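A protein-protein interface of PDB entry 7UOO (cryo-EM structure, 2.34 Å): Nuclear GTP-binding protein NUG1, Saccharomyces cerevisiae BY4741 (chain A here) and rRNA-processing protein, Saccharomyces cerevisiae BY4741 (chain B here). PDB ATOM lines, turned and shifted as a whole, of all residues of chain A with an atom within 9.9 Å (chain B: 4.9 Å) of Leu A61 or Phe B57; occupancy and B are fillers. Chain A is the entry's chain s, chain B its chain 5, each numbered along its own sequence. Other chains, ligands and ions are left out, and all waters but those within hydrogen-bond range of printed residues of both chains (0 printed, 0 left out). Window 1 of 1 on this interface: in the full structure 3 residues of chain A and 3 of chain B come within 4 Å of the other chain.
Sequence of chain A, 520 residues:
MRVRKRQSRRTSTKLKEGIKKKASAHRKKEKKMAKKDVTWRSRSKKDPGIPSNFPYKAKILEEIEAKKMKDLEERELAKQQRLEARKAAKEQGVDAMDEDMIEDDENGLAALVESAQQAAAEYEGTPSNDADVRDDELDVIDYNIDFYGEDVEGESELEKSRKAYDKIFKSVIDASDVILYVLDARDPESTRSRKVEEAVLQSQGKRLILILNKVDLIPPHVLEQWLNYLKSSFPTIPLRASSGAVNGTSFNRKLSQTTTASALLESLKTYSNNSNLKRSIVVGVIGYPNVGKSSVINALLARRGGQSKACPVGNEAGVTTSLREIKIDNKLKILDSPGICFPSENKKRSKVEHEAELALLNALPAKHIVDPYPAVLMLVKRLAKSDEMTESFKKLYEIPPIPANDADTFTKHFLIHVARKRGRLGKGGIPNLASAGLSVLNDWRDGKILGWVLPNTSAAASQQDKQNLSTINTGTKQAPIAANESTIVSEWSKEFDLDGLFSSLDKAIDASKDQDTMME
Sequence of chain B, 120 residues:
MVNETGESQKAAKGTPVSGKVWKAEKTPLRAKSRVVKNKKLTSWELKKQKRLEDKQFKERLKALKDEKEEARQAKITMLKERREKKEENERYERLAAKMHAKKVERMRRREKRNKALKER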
ATOM      1  N   GLY A  49     -18.064  -0.595  -7.676  1.00  0.00           N
ATOM      2  CA  GLY A  49     -19.035  -0.286  -8.708  1.00  0.00           C
ATOM      3  C   GLY A  49     -20.322  -1.085  -8.565  1.00  0.00           C
ATOM      4  O   GLY A  49     -20.725  -1.481  -7.471  1.00  0.00           O
ATOM      5  N   ILE A  50     -20.968  -1.314  -9.698  1.00  0.00           N
ATOM      6  CA  ILE A  50     -22.265  -1.985  -9.756  1.00  0.00           C
ATOM      7  C   ILE A  50     -22.031  -3.457 -10.076  1.00  0.00           C
ATOM      8  O   ILE A  50     -21.334  -3.759 -11.054  1.00  0.00           O
ATOM      9  CB  ILE A  50     -23.183  -1.341 -10.809  1.00  0.00           C
ATOM     10  CG1 ILE A  50     -23.182   0.181 -10.655  1.00  0.00           C
ATOM     11  CG2 ILE A  50     -24.595  -1.886 -10.692  1.00  0.00           C
ATOM     12  CD1 ILE A  50     -23.798   0.909 -11.823  1.00  0.00           C
ATOM     13  N   PRO A  51     -22.574  -4.388  -9.289  1.00  0.00           N
ATOM     14  CA  PRO A  51     -22.432  -5.808  -9.624  1.00  0.00           C
ATOM     15  C   PRO A  51     -23.135  -6.143 -10.931  1.00  0.00           C
ATOM     16  O   PRO A  51     -24.179  -5.579 -11.265  1.00  0.00           O
ATOM     17  CB  PRO A  51     -23.088  -6.521  -8.435  1.00  0.00           C
ATOM     18  CG  PRO A  51     -24.033  -5.517  -7.873  1.00  0.00           C
ATOM     19  CD  PRO A  51     -23.370  -4.186  -8.069  1.00  0.00           C
ATOM     20  N   SER A  52     -22.544  -7.078 -11.674  1.00  0.00           N
ATOM     21  CA  SER A  52     -23.054  -7.416 -12.996  1.00  0.00           C
ATOM     22  C   SER A  52     -24.354  -8.206 -12.938  1.00  0.00           C
ATOM     23  O   SER A  52     -25.113  -8.196 -13.912  1.00  0.00           O
ATOM     24  CB  SER A  52     -22.002  -8.203 -13.775  1.00  0.00           C
ATOM     25  OG  SER A  52     -20.805  -7.456 -13.902  1.00  0.00           O
ATOM     26  N   ASN A  53     -24.631  -8.879 -11.825  1.00  0.00           N
ATOM     27  CA  ASN A  53     -25.814  -9.720 -11.707  1.00  0.00           C
ATOM     28  C   ASN A  53     -27.067  -8.953 -11.303  1.00  0.00           C
ATOM     29  O   ASN A  53     -28.148  -9.547 -11.265  1.00  0.00           O
ATOM     30  CB  ASN A  53     -25.558 -10.845 -10.700  1.00  0.00           C
ATOM     31  CG  ASN A  53     -24.486 -11.811 -11.166  1.00  0.00           C
ATOM     32  OD1 ASN A  53     -23.420 -11.913 -10.559  1.00  0.00           O
ATOM     33  ND2 ASN A  53     -24.766 -12.527 -12.247  1.00  0.00           N
ATOM     34  N   PHE A  54     -26.956  -7.665 -10.994  1.00  0.00           N
ATOM     35  CA  PHE A  54     -28.138  -6.887 -10.657  1.00  0.00           C
ATOM     36  C   PHE A  54     -28.987  -6.664 -11.907  1.00  0.00           C
ATOM     37  O   PHE A  54     -28.446  -6.426 -12.991  1.00  0.00           O
ATOM     38  CB  PHE A  54     -27.742  -5.545 -10.040  1.00  0.00           C
ATOM     39  CG  PHE A  54     -28.817  -4.931  -9.188  1.00  0.00           C
ATOM     40  CD1 PHE A  54     -28.963  -5.304  -7.863  1.00  0.00           C
ATOM     41  CD2 PHE A  54     -29.679  -3.981  -9.711  1.00  0.00           C
ATOM     42  CE1 PHE A  54     -29.949  -4.747  -7.075  1.00  0.00           C
ATOM     43  CE2 PHE A  54     -30.668  -3.419  -8.927  1.00  0.00           C
ATOM     44  CZ  PHE A  54     -30.803  -3.803  -7.606  1.00  0.00           C
ATOM     45  N   PRO A  55     -30.315  -6.756 -11.799  1.00  0.00           N
ATOM     46  CA  PRO A  55     -31.141  -6.605 -13.007  1.00  0.00           C
ATOM     47  C   PRO A  55     -31.242  -5.175 -13.517  1.00  0.00           C
ATOM     48  O   PRO A  55     -31.149  -4.958 -14.730  1.00  0.00           O
ATOM     49  CB  PRO A  55     -32.504  -7.154 -12.565  1.00  0.00           C
ATOM     50  CG  PRO A  55     -32.517  -6.977 -11.089  1.00  0.00           C
ATOM     51  CD  PRO A  55     -31.105  -7.194 -10.637  1.00  0.00           C
ATOM     52  N   TYR A  56     -31.438  -4.194 -12.639  1.00  0.00           N
ATOM     53  CA  TYR A  56     -31.668  -2.818 -13.088  1.00  0.00           C
ATOM     54  C   TYR A  56     -30.379  -1.998 -13.134  1.00  0.00           C
ATOM     55  O   TYR A  56     -30.323  -0.845 -12.690  1.00  0.00           O
ATOM     56  CB  TYR A  56     -32.709  -2.160 -12.193  1.00  0.00           C
ATOM     57  CG  TYR A  56     -33.915  -3.033 -11.928  1.00  0.00           C
ATOM     58  CD1 TYR A  56     -34.799  -3.358 -12.947  1.00  0.00           C
ATOM     59  CD2 TYR A  56     -34.171  -3.529 -10.657  1.00  0.00           C
ATOM     60  CE1 TYR A  56     -35.899  -4.157 -12.710  1.00  0.00           C
ATOM     61  CE2 TYR A  56     -35.268  -4.326 -10.409  1.00  0.00           C
ATOM     62  CZ  TYR A  56     -36.130  -4.638 -11.440  1.00  0.00           C
ATOM     63  OH  TYR A  56     -37.226  -5.430 -11.197  1.00  0.00           O
ATOM     64  N   LYS A  57     -29.343  -2.584 -13.739  1.00  0.00           N
ATOM     65  CA  LYS A  57     -28.087  -1.866 -13.930  1.00  0.00           C
ATOM     66  C   LYS A  57     -28.268  -0.692 -14.878  1.00  0.00           C
ATOM     67  O   LYS A  57     -27.670   0.371 -14.682  1.00  0.00           O
ATOM     68  CB  LYS A  57     -27.011  -2.805 -14.469  1.00  0.00           C
ATOM     69  CG  LYS A  57     -26.558  -3.883 -13.515  1.00  0.00           C
ATOM     70  CD  LYS A  57     -25.609  -4.840 -14.218  1.00  0.00           C
ATOM     71  CE  LYS A  57     -26.228  -5.382 -15.499  1.00  0.00           C
ATOM     72  NZ  LYS A  57     -25.283  -6.243 -16.257  1.00  0.00           N
ATOM     73  N   ALA A  58     -29.074  -0.877 -15.928  1.00  0.00           N
ATOM     74  CA  ALA A  58     -29.324   0.204 -16.873  1.00  0.00           C
ATOM     75  C   ALA A  58     -30.022   1.375 -16.198  1.00  0.00           C
ATOM     76  O   ALA A  58     -29.677   2.534 -16.443  1.00  0.00           O
ATOM     77  CB  ALA A  58     -30.149  -0.308 -18.052  1.00  0.00           C
ATOM     78  N   LYS A  59     -31.002   1.091 -15.334  1.00  0.00           N
ATOM     79  CA  LYS A  59     -31.673   2.160 -14.601  1.00  0.00           C
ATOM     80  C   LYS A  59     -30.715   2.867 -13.650  1.00  0.00           C
ATOM     81  O   LYS A  59     -30.746   4.099 -13.538  1.00  0.00           O
ATOM     82  CB  LYS A  59     -32.877   1.607 -13.840  1.00  0.00           C
ATOM     83  CG  LYS A  59     -33.979   1.067 -14.734  1.00  0.00           C
ATOM     84  CD  LYS A  59     -35.160   0.570 -13.920  1.00  0.00           C
ATOM     85  CE  LYS A  59     -36.220  -0.056 -14.812  1.00  0.00           C
ATOM     86  NZ  LYS A  59     -35.689  -1.221 -15.568  1.00  0.00           N
ATOM     87  N   ILE A  60     -29.855   2.108 -12.960  1.00  0.00           N
ATOM     88  CA  ILE A  60     -28.877   2.732 -12.067  1.00  0.00           C
ATOM     89  C   ILE A  60     -27.932   3.639 -12.851  1.00  0.00           C
ATOM     90  O   ILE A  60     -27.625   4.762 -12.425  1.00  0.00           O
ATOM     91  CB  ILE A  60     -28.104   1.655 -11.281  1.00  0.00           C
ATOM     92  CG1 ILE A  60     -29.037   0.913 -10.322  1.00  0.00           C
ATOM     93  CG2 ILE A  60     -26.954   2.277 -10.503  1.00  0.00           C
ATOM     94  CD1 ILE A  60     -29.508   1.748  -9.158  1.00  0.00           C
ATOM     95  N   LEU A  61     -27.465   3.169 -14.010  1.00  0.00           N
ATOM     96  CA  LEU A  61     -26.550   3.961 -14.829  1.00  0.00           C
ATOM     97  C   LEU A  61     -27.228   5.215 -15.370  1.00  0.00           C
ATOM     98  O   LEU A  61     -26.617   6.289 -15.405  1.00  0.00           O
ATOM     99  CB  LEU A  61     -25.999   3.108 -15.970  1.00  0.00           C
ATOM    100  CG  LEU A  61     -24.835   3.709 -16.761  1.00  0.00           C
ATOM    101  CD1 LEU A  61     -23.673   4.035 -15.836  1.00  0.00           C
ATOM    102  CD2 LEU A  61     -24.393   2.765 -17.866  1.00  0.00           C
ATOM    103  N   GLU A  62     -28.489   5.101 -15.798  1.00  0.00           N
ATOM    104  CA  GLU A  62     -29.220   6.276 -16.260  1.00  0.00           C
ATOM    105  C   GLU A  62     -29.398   7.294 -15.140  1.00  0.00           C
ATOM    106  O   GLU A  62     -29.223   8.500 -15.355  1.00  0.00           O
ATOM    107  CB  GLU A  62     -30.578   5.861 -16.824  1.00  0.00           C
ATOM    108  CG  GLU A  62     -30.506   5.111 -18.142  1.00  0.00           C
ATOM    109  CD  GLU A  62     -31.716   4.226 -18.371  1.00  0.00           C
ATOM    110  OE1 GLU A  62     -32.511   4.049 -17.424  1.00  0.00           O
ATOM    111  OE2 GLU A  62     -31.872   3.705 -19.495  1.00  0.00           O
ATOM    112  N   GLU A  63     -29.734   6.823 -13.936  1.00  0.00           N
ATOM    113  CA  GLU A  63     -29.913   7.735 -12.810  1.00  0.00           C
ATOM    114  C   GLU A  63     -28.608   8.434 -12.443  1.00  0.00           C
ATOM    115  O   GLU A  63     -28.597   9.643 -12.186  1.00  0.00           O
ATOM    116  CB  GLU A  63     -30.478   6.984 -11.605  1.00  0.00           C
ATOM    117  CG  GLU A  63     -31.920   6.532 -11.777  1.00  0.00           C
ATOM    118  CD  GLU A  63     -32.457   5.817 -10.551  1.00  0.00           C
ATOM    119  OE1 GLU A  63     -31.765   5.816  -9.512  1.00  0.00           O
ATOM    120  OE2 GLU A  63     -33.570   5.258 -10.628  1.00  0.00           O
ATOM    121  N   ILE A  64     -27.494   7.695 -12.424  1.00  0.00           N
ATOM    122  CA  ILE A  64     -26.230   8.326 -12.050  1.00  0.00           C
ATOM    123  C   ILE A  64     -25.750   9.275 -13.147  1.00  0.00           C
ATOM    124  O   ILE A  64     -25.149  10.316 -12.850  1.00  0.00           O
ATOM    125  CB  ILE A  64     -25.168   7.268 -11.676  1.00  0.00           C
ATOM    126  CG1 ILE A  64     -23.965   7.931 -11.005  1.00  0.00           C
ATOM    127  CG2 ILE A  64     -24.711   6.467 -12.878  1.00  0.00           C
ATOM    128  CD1 ILE A  64     -24.311   8.685  -9.740  1.00  0.00           C
ATOM    129  N   GLU A  65     -26.024   8.964 -14.421  1.00  0.00           N
ATOM    130  CA  GLU A  65     -25.690   9.898 -15.492  1.00  0.00           C
ATOM    131  C   GLU A  65     -26.511  11.178 -15.388  1.00  0.00           C
ATOM    132  O   GLU A  65     -25.984  12.278 -15.593  1.00  0.00           O
ATOM    133  CB  GLU A  65     -25.895   9.239 -16.855  1.00  0.00           C
ATOM    134  CG  GLU A  65     -24.790   8.277 -17.257  1.00  0.00           C
ATOM    135  CD  GLU A  65     -25.050   7.623 -18.600  1.00  0.00           C
ATOM    136  OE1 GLU A  65     -26.151   7.820 -19.155  1.00  0.00           O
ATOM    137  OE2 GLU A  65     -24.153   6.915 -19.102  1.00  0.00           O
ATOM    138  N   ALA A  66     -27.802  11.054 -15.069  1.00  0.00           N
ATOM    139  CA  ALA A  66     -28.632  12.239 -14.872  1.00  0.00           C
ATOM    140  C   ALA A  66     -28.140  13.070 -13.694  1.00  0.00           C
ATOM    141  O   ALA A  66     -28.113  14.306 -13.761  1.00  0.00           O
ATOM    142  CB  ALA A  66     -30.091  11.830 -14.669  1.00  0.00           C
ATOM    143  N   LYS A  67     -27.742  12.407 -12.604  1.00  0.00           N
ATOM    144  CA  LYS A  67     -27.211  13.129 -11.451  1.00  0.00           C
ATOM    145  C   LYS A  67     -25.915  13.855 -11.797  1.00  0.00           C
ATOM    146  O   LYS A  67     -25.701  14.992 -11.360  1.00  0.00           O
ATOM    147  CB  LYS A  67     -26.997  12.170 -10.280  1.00  0.00           C
ATOM    148  CG  LYS A  67     -28.286  11.675  -9.645  1.00  0.00           C
ATOM    149  CD  LYS A  67     -28.011  10.652  -8.553  1.00  0.00           C
ATOM    150  CE  LYS A  67     -29.302  10.172  -7.909  1.00  0.00           C
ATOM    151  NZ  LYS A  67     -29.064   9.110  -6.891  1.00  0.00           N
ATOM    152  N   LYS A  68     -25.038  13.213 -12.576  1.00  0.00           N
ATOM    153  CA  LYS A  68     -23.812  13.881 -13.011  1.00  0.00           C
ATOM    154  C   LYS A  68     -24.121  15.091 -13.883  1.00  0.00           C
ATOM    155  O   LYS A  68     -23.520  16.160 -13.711  1.00  0.00           O
ATOM    156  CB  LYS A  68     -22.909  12.904 -13.766  1.00  0.00           C
ATOM    157  CG  LYS A  68     -22.263  11.833 -12.906  1.00  0.00           C
ATOM    158  CD  LYS A  68     -21.257  11.021 -13.712  1.00  0.00           C
ATOM    159  CE  LYS A  68     -20.787   9.792 -12.949  1.00  0.00           C
ATOM    160  NZ  LYS A  68     -19.808   8.986 -13.734  1.00  0.00           N
ATOM    161  N   MET A  69     -25.064  14.945 -14.820  1.00  0.00           N
ATOM    162  CA  MET A  69     -25.416  16.055 -15.701  1.00  0.00           C
ATOM    163  C   MET A  69     -26.033  17.213 -14.929  1.00  0.00           C
ATOM    164  O   MET A  69     -25.826  18.377 -15.290  1.00  0.00           O
ATOM    165  CB  MET A  69     -26.371  15.580 -16.797  1.00  0.00           C
ATOM    166  CG  MET A  69     -25.736  14.639 -17.806  1.00  0.00           C
ATOM    167  SD  MET A  69     -26.865  14.158 -19.125  1.00  0.00           S
ATOM    168  CE  MET A  69     -27.138  15.735 -19.928  1.00  0.00           C
ATOM    169  N   GLU B  53     -28.769  -6.608 -24.575  1.00  0.00           N
ATOM    170  CA  GLU B  53     -28.887  -5.508 -23.622  1.00  0.00           C
ATOM    171  C   GLU B  53     -27.682  -5.446 -22.693  1.00  0.00           C
ATOM    172  O   GLU B  53     -27.163  -4.358 -22.404  1.00  0.00           O
ATOM    173  CB  GLU B  53     -30.174  -5.651 -22.811  1.00  0.00           C
ATOM    174  CG  GLU B  53     -31.446  -5.382 -23.590  1.00  0.00           C
ATOM    175  CD  GLU B  53     -32.690  -5.657 -22.769  1.00  0.00           C
ATOM    176  OE1 GLU B  53     -32.597  -6.426 -21.790  1.00  0.00           O
ATOM    177  OE2 GLU B  53     -33.760  -5.102 -23.099  1.00  0.00           O
ATOM    178  N   ASP B  54     -27.227  -6.606 -22.210  1.00  0.00           N
ATOM    179  CA  ASP B  54     -26.056  -6.646 -21.341  1.00  0.00           C
ATOM    180  C   ASP B  54     -24.811  -6.162 -22.071  1.00  0.00           C
ATOM    181  O   ASP B  54     -23.988  -5.442 -21.494  1.00  0.00           O
ATOM    182  CB  ASP B  54     -25.851  -8.062 -20.807  1.00  0.00           C
ATOM    183  CG  ASP B  54     -24.753  -8.137 -19.768  1.00  0.00           C
ATOM    184  OD1 ASP B  54     -24.941  -7.585 -18.663  1.00  0.00           O
ATOM    185  OD2 ASP B  54     -23.701  -8.745 -20.054  1.00  0.00           O
ATOM    186  N   LYS B  55     -24.654  -6.545 -23.342  1.00  0.00           N
ATOM    187  CA  LYS B  55     -23.506  -6.083 -24.115  1.00  0.00           C
ATOM    188  C   LYS B  55     -23.538  -4.572 -24.317  1.00  0.00           C
ATOM    189  O   LYS B  55     -22.499  -3.904 -24.227  1.00  0.00           O
ATOM    190  CB  LYS B  55     -23.451  -6.805 -25.460  1.00  0.00           C
ATOM    191  CG  LYS B  55     -22.919  -8.221 -25.360  1.00  0.00           C
ATOM    192  CD  LYS B  55     -22.963  -8.940 -26.695  1.00  0.00           C
ATOM    193  CE  LYS B  55     -22.272 -10.288 -26.597  1.00  0.00           C
ATOM    194  NZ  LYS B  55     -22.775 -11.076 -25.439  1.00  0.00           N
ATOM    195  N   GLN B  56     -24.722  -4.014 -24.594  1.00  0.00           N
ATOM    196  CA  GLN B  56     -24.832  -2.565 -24.737  1.00  0.00           C
ATOM    197  C   GLN B  56     -24.497  -1.849 -23.433  1.00  0.00           C
ATOM    198  O   GLN B  56     -23.786  -0.833 -23.436  1.00  0.00           O
ATOM    199  CB  GLN B  56     -26.230  -2.182 -25.218  1.00  0.00           C
ATOM    200  CG  GLN B  56     -26.422  -2.322 -26.716  1.00  0.00           C
ATOM    201  CD  GLN B  56     -27.493  -1.395 -27.250  1.00  0.00           C
ATOM    202  OE1 GLN B  56     -28.373  -0.954 -26.510  1.00  0.00           O
ATOM    203  NE2 GLN B  56     -27.418  -1.084 -28.538  1.00  0.00           N
ATOM    204  N   PHE B  57     -24.989  -2.371 -22.305  1.00  0.00           N
ATOM    205  CA  PHE B  57     -24.653  -1.778 -21.011  1.00  0.00           C
ATOM    206  C   PHE B  57     -23.153  -1.834 -20.753  1.00  0.00           C
ATOM    207  O   PHE B  57     -22.558  -0.854 -20.281  1.00  0.00           O
ATOM    208  CB  PHE B  57     -25.413  -2.486 -19.888  1.00  0.00           C
ATOM    209  CG  PHE B  57     -24.959  -2.093 -18.506  1.00  0.00           C
ATOM    210  CD1 PHE B  57     -25.413  -0.923 -17.922  1.00  0.00           C
ATOM    211  CD2 PHE B  57     -24.078  -2.893 -17.793  1.00  0.00           C
ATOM    212  CE1 PHE B  57     -24.998  -0.558 -16.655  1.00  0.00           C
ATOM    213  CE2 PHE B  57     -23.659  -2.528 -16.528  1.00  0.00           C
ATOM    214  CZ  PHE B  57     -24.119  -1.359 -15.959  1.00  0.00           C
ATOM    215  N   LYS B  58     -22.527  -2.974 -21.053  1.00  0.00           N
ATOM    216  CA  LYS B  58     -21.103  -3.129 -20.781  1.00  0.00           C
ATOM    217  C   LYS B  58     -20.266  -2.200 -21.649  1.00  0.00           C
ATOM    218  O   LYS B  58     -19.297  -1.604 -21.165  1.00  0.00           O
ATOM    219  CB  LYS B  58     -20.681  -4.586 -20.978  1.00  0.00           C
ATOM    220  CG  LYS B  58     -21.213  -5.524 -19.906  1.00  0.00           C
ATOM    221  CD  LYS B  58     -20.781  -6.958 -20.146  1.00  0.00           C
ATOM    222  CE  LYS B  58     -19.308  -7.150 -19.835  1.00  0.00           C
ATOM    223  NZ  LYS B  58     -19.017  -6.902 -18.397  1.00  0.00           N
ATOM    224  N   GLU B  59     -20.627  -2.043 -22.927  1.00  0.00           N
ATOM    225  CA  GLU B  59     -19.849  -1.140 -23.771  1.00  0.00           C
ATOM    226  C   GLU B  59     -20.068   0.321 -23.385  1.00  0.00           C
ATOM    227  O   GLU B  59     -19.128   1.121 -23.461  1.00  0.00           O
ATOM    228  CB  GLU B  59     -20.159  -1.372 -25.252  1.00  0.00           C
ATOM    229  CG  GLU B  59     -21.578  -1.073 -25.687  1.00  0.00           C
ATOM    230  CD  GLU B  59     -21.777  -1.251 -27.177  1.00  0.00           C
ATOM    231  OE1 GLU B  59     -20.776  -1.203 -27.921  1.00  0.00           O
ATOM    232  OE2 GLU B  59     -22.934  -1.442 -27.604  1.00  0.00           O
ATOM    233  N   ARG B  60     -21.275   0.685 -22.935  1.00  0.00           N
ATOM    234  CA  ARG B  60     -21.490   2.047 -22.446  1.00  0.00           C
ATOM    235  C   ARG B  60     -20.652   2.329 -21.200  1.00  0.00           C
ATOM    236  O   ARG B  60     -20.012   3.388 -21.092  1.00  0.00           O
ATOM    237  CB  ARG B  60     -22.974   2.268 -22.157  1.00  0.00           C
ATOM    238  CG  ARG B  60     -23.345   3.692 -21.768  1.00  0.00           C
ATOM    239  CD  ARG B  60     -23.634   4.565 -22.984  1.00  0.00           C
ATOM    240  NE  ARG B  60     -22.432   4.901 -23.740  1.00  0.00           N
ATOM    241  CZ  ARG B  60     -22.412   5.693 -24.803  1.00  0.00           C
ATOM    242  NH1 ARG B  60     -23.516   6.251 -25.270  1.00  0.00           N
ATOM    243  NH2 ARG B  60     -21.253   5.934 -25.409  1.00  0.00           N
ATOM    244  N   LEU B  61     -20.633   1.383 -20.257  1.00  0.00           N
ATOM    245  CA  LEU B  61     -19.831   1.556 -19.049  1.00  0.00           C
ATOM    246  C   LEU B  61     -18.344   1.606 -19.379  1.00  0.00           C
ATOM    247  O   LEU B  61     -17.590   2.383 -18.777  1.00  0.00           O
ATOM    248  CB  LEU B  61     -20.127   0.425 -18.064  1.00  0.00           C
ATOM    249  CG  LEU B  61     -19.626   0.598 -16.631  1.00  0.00           C
ATOM    250  CD1 LEU B  61     -20.329   1.762 -15.959  1.00  0.00           C
ATOM    251  CD2 LEU B  61     -19.832  -0.682 -15.839  1.00  0.00           C
ATOM    252  N   LEU B  64     -17.530   5.054 -20.690  1.00  0.00           N
ATOM    253  CA  LEU B  64     -17.443   6.024 -19.599  1.00  0.00           C
ATOM    254  C   LEU B  64     -16.134   5.882 -18.822  1.00  0.00           C
ATOM    255  O   LEU B  64     -15.482   6.884 -18.495  1.00  0.00           O
ATOM    256  CB  LEU B  64     -18.639   5.872 -18.662  1.00  0.00           C
ATOM    257  CG  LEU B  64     -20.004   6.226 -19.251  1.00  0.00           C
ATOM    258  CD1 LEU B  64     -21.090   6.081 -18.199  1.00  0.00           C
ATOM    259  CD2 LEU B  64     -19.988   7.632 -19.830  1.00  0.00           C
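The side-chain carboxylate (OD1) of Asp B54 lies within salt-bridge range of the side-chain amino group (NZ) of Lys A57.
The side-chain amino group of Lys A57 is in hydrogen-bond range of the backbone carbonyl oxygen of Ser A52.
Among the printed residues, pairs that only touch across the chains: Glu A65 with Leu B64 (3.3 Å), Lys A57 with Phe B57 (3.4 Å) and Leu A61 with Phe B57 (3.6 Å).
Of the printed residues of chain B, Leu A61 touches Phe B57.
Of chain A, only Lys A57 and Leu A61 come within 4 Å of Phe B57.
Of the printed residues of chain B, Glu A65 touches Leu B64 (3.3 Å).
Printed residues of chain A within 4 Å of Leu B64: Glu A65 (3.3 Å).
Printed residues of chain A within 4 Å of Asp B54: Lys A57.
Of the printed residues of chain B, Lys A57 touches Asp B54 and Phe B57.
Lys B58 touches none of the printed residues of chain A.
Gln B56 touches none of the printed residues of chain A.
Of the 21 printed residues of chain A, 3 touch a printed residue of chain B.
Hydrophobic or aromatic side chains of chain A within 4 Å of the printed part of chain B: Leu A61.
Hydrophobic or aromatic side chains of chain B within 4 Å of the printed part of chain A: Phe B57 and Leu B64.
Along chain B the printed residues that touch a printed residue of chain A span positions 54 to 64.
Among the printed residues, 4 pairs touch across the chains.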
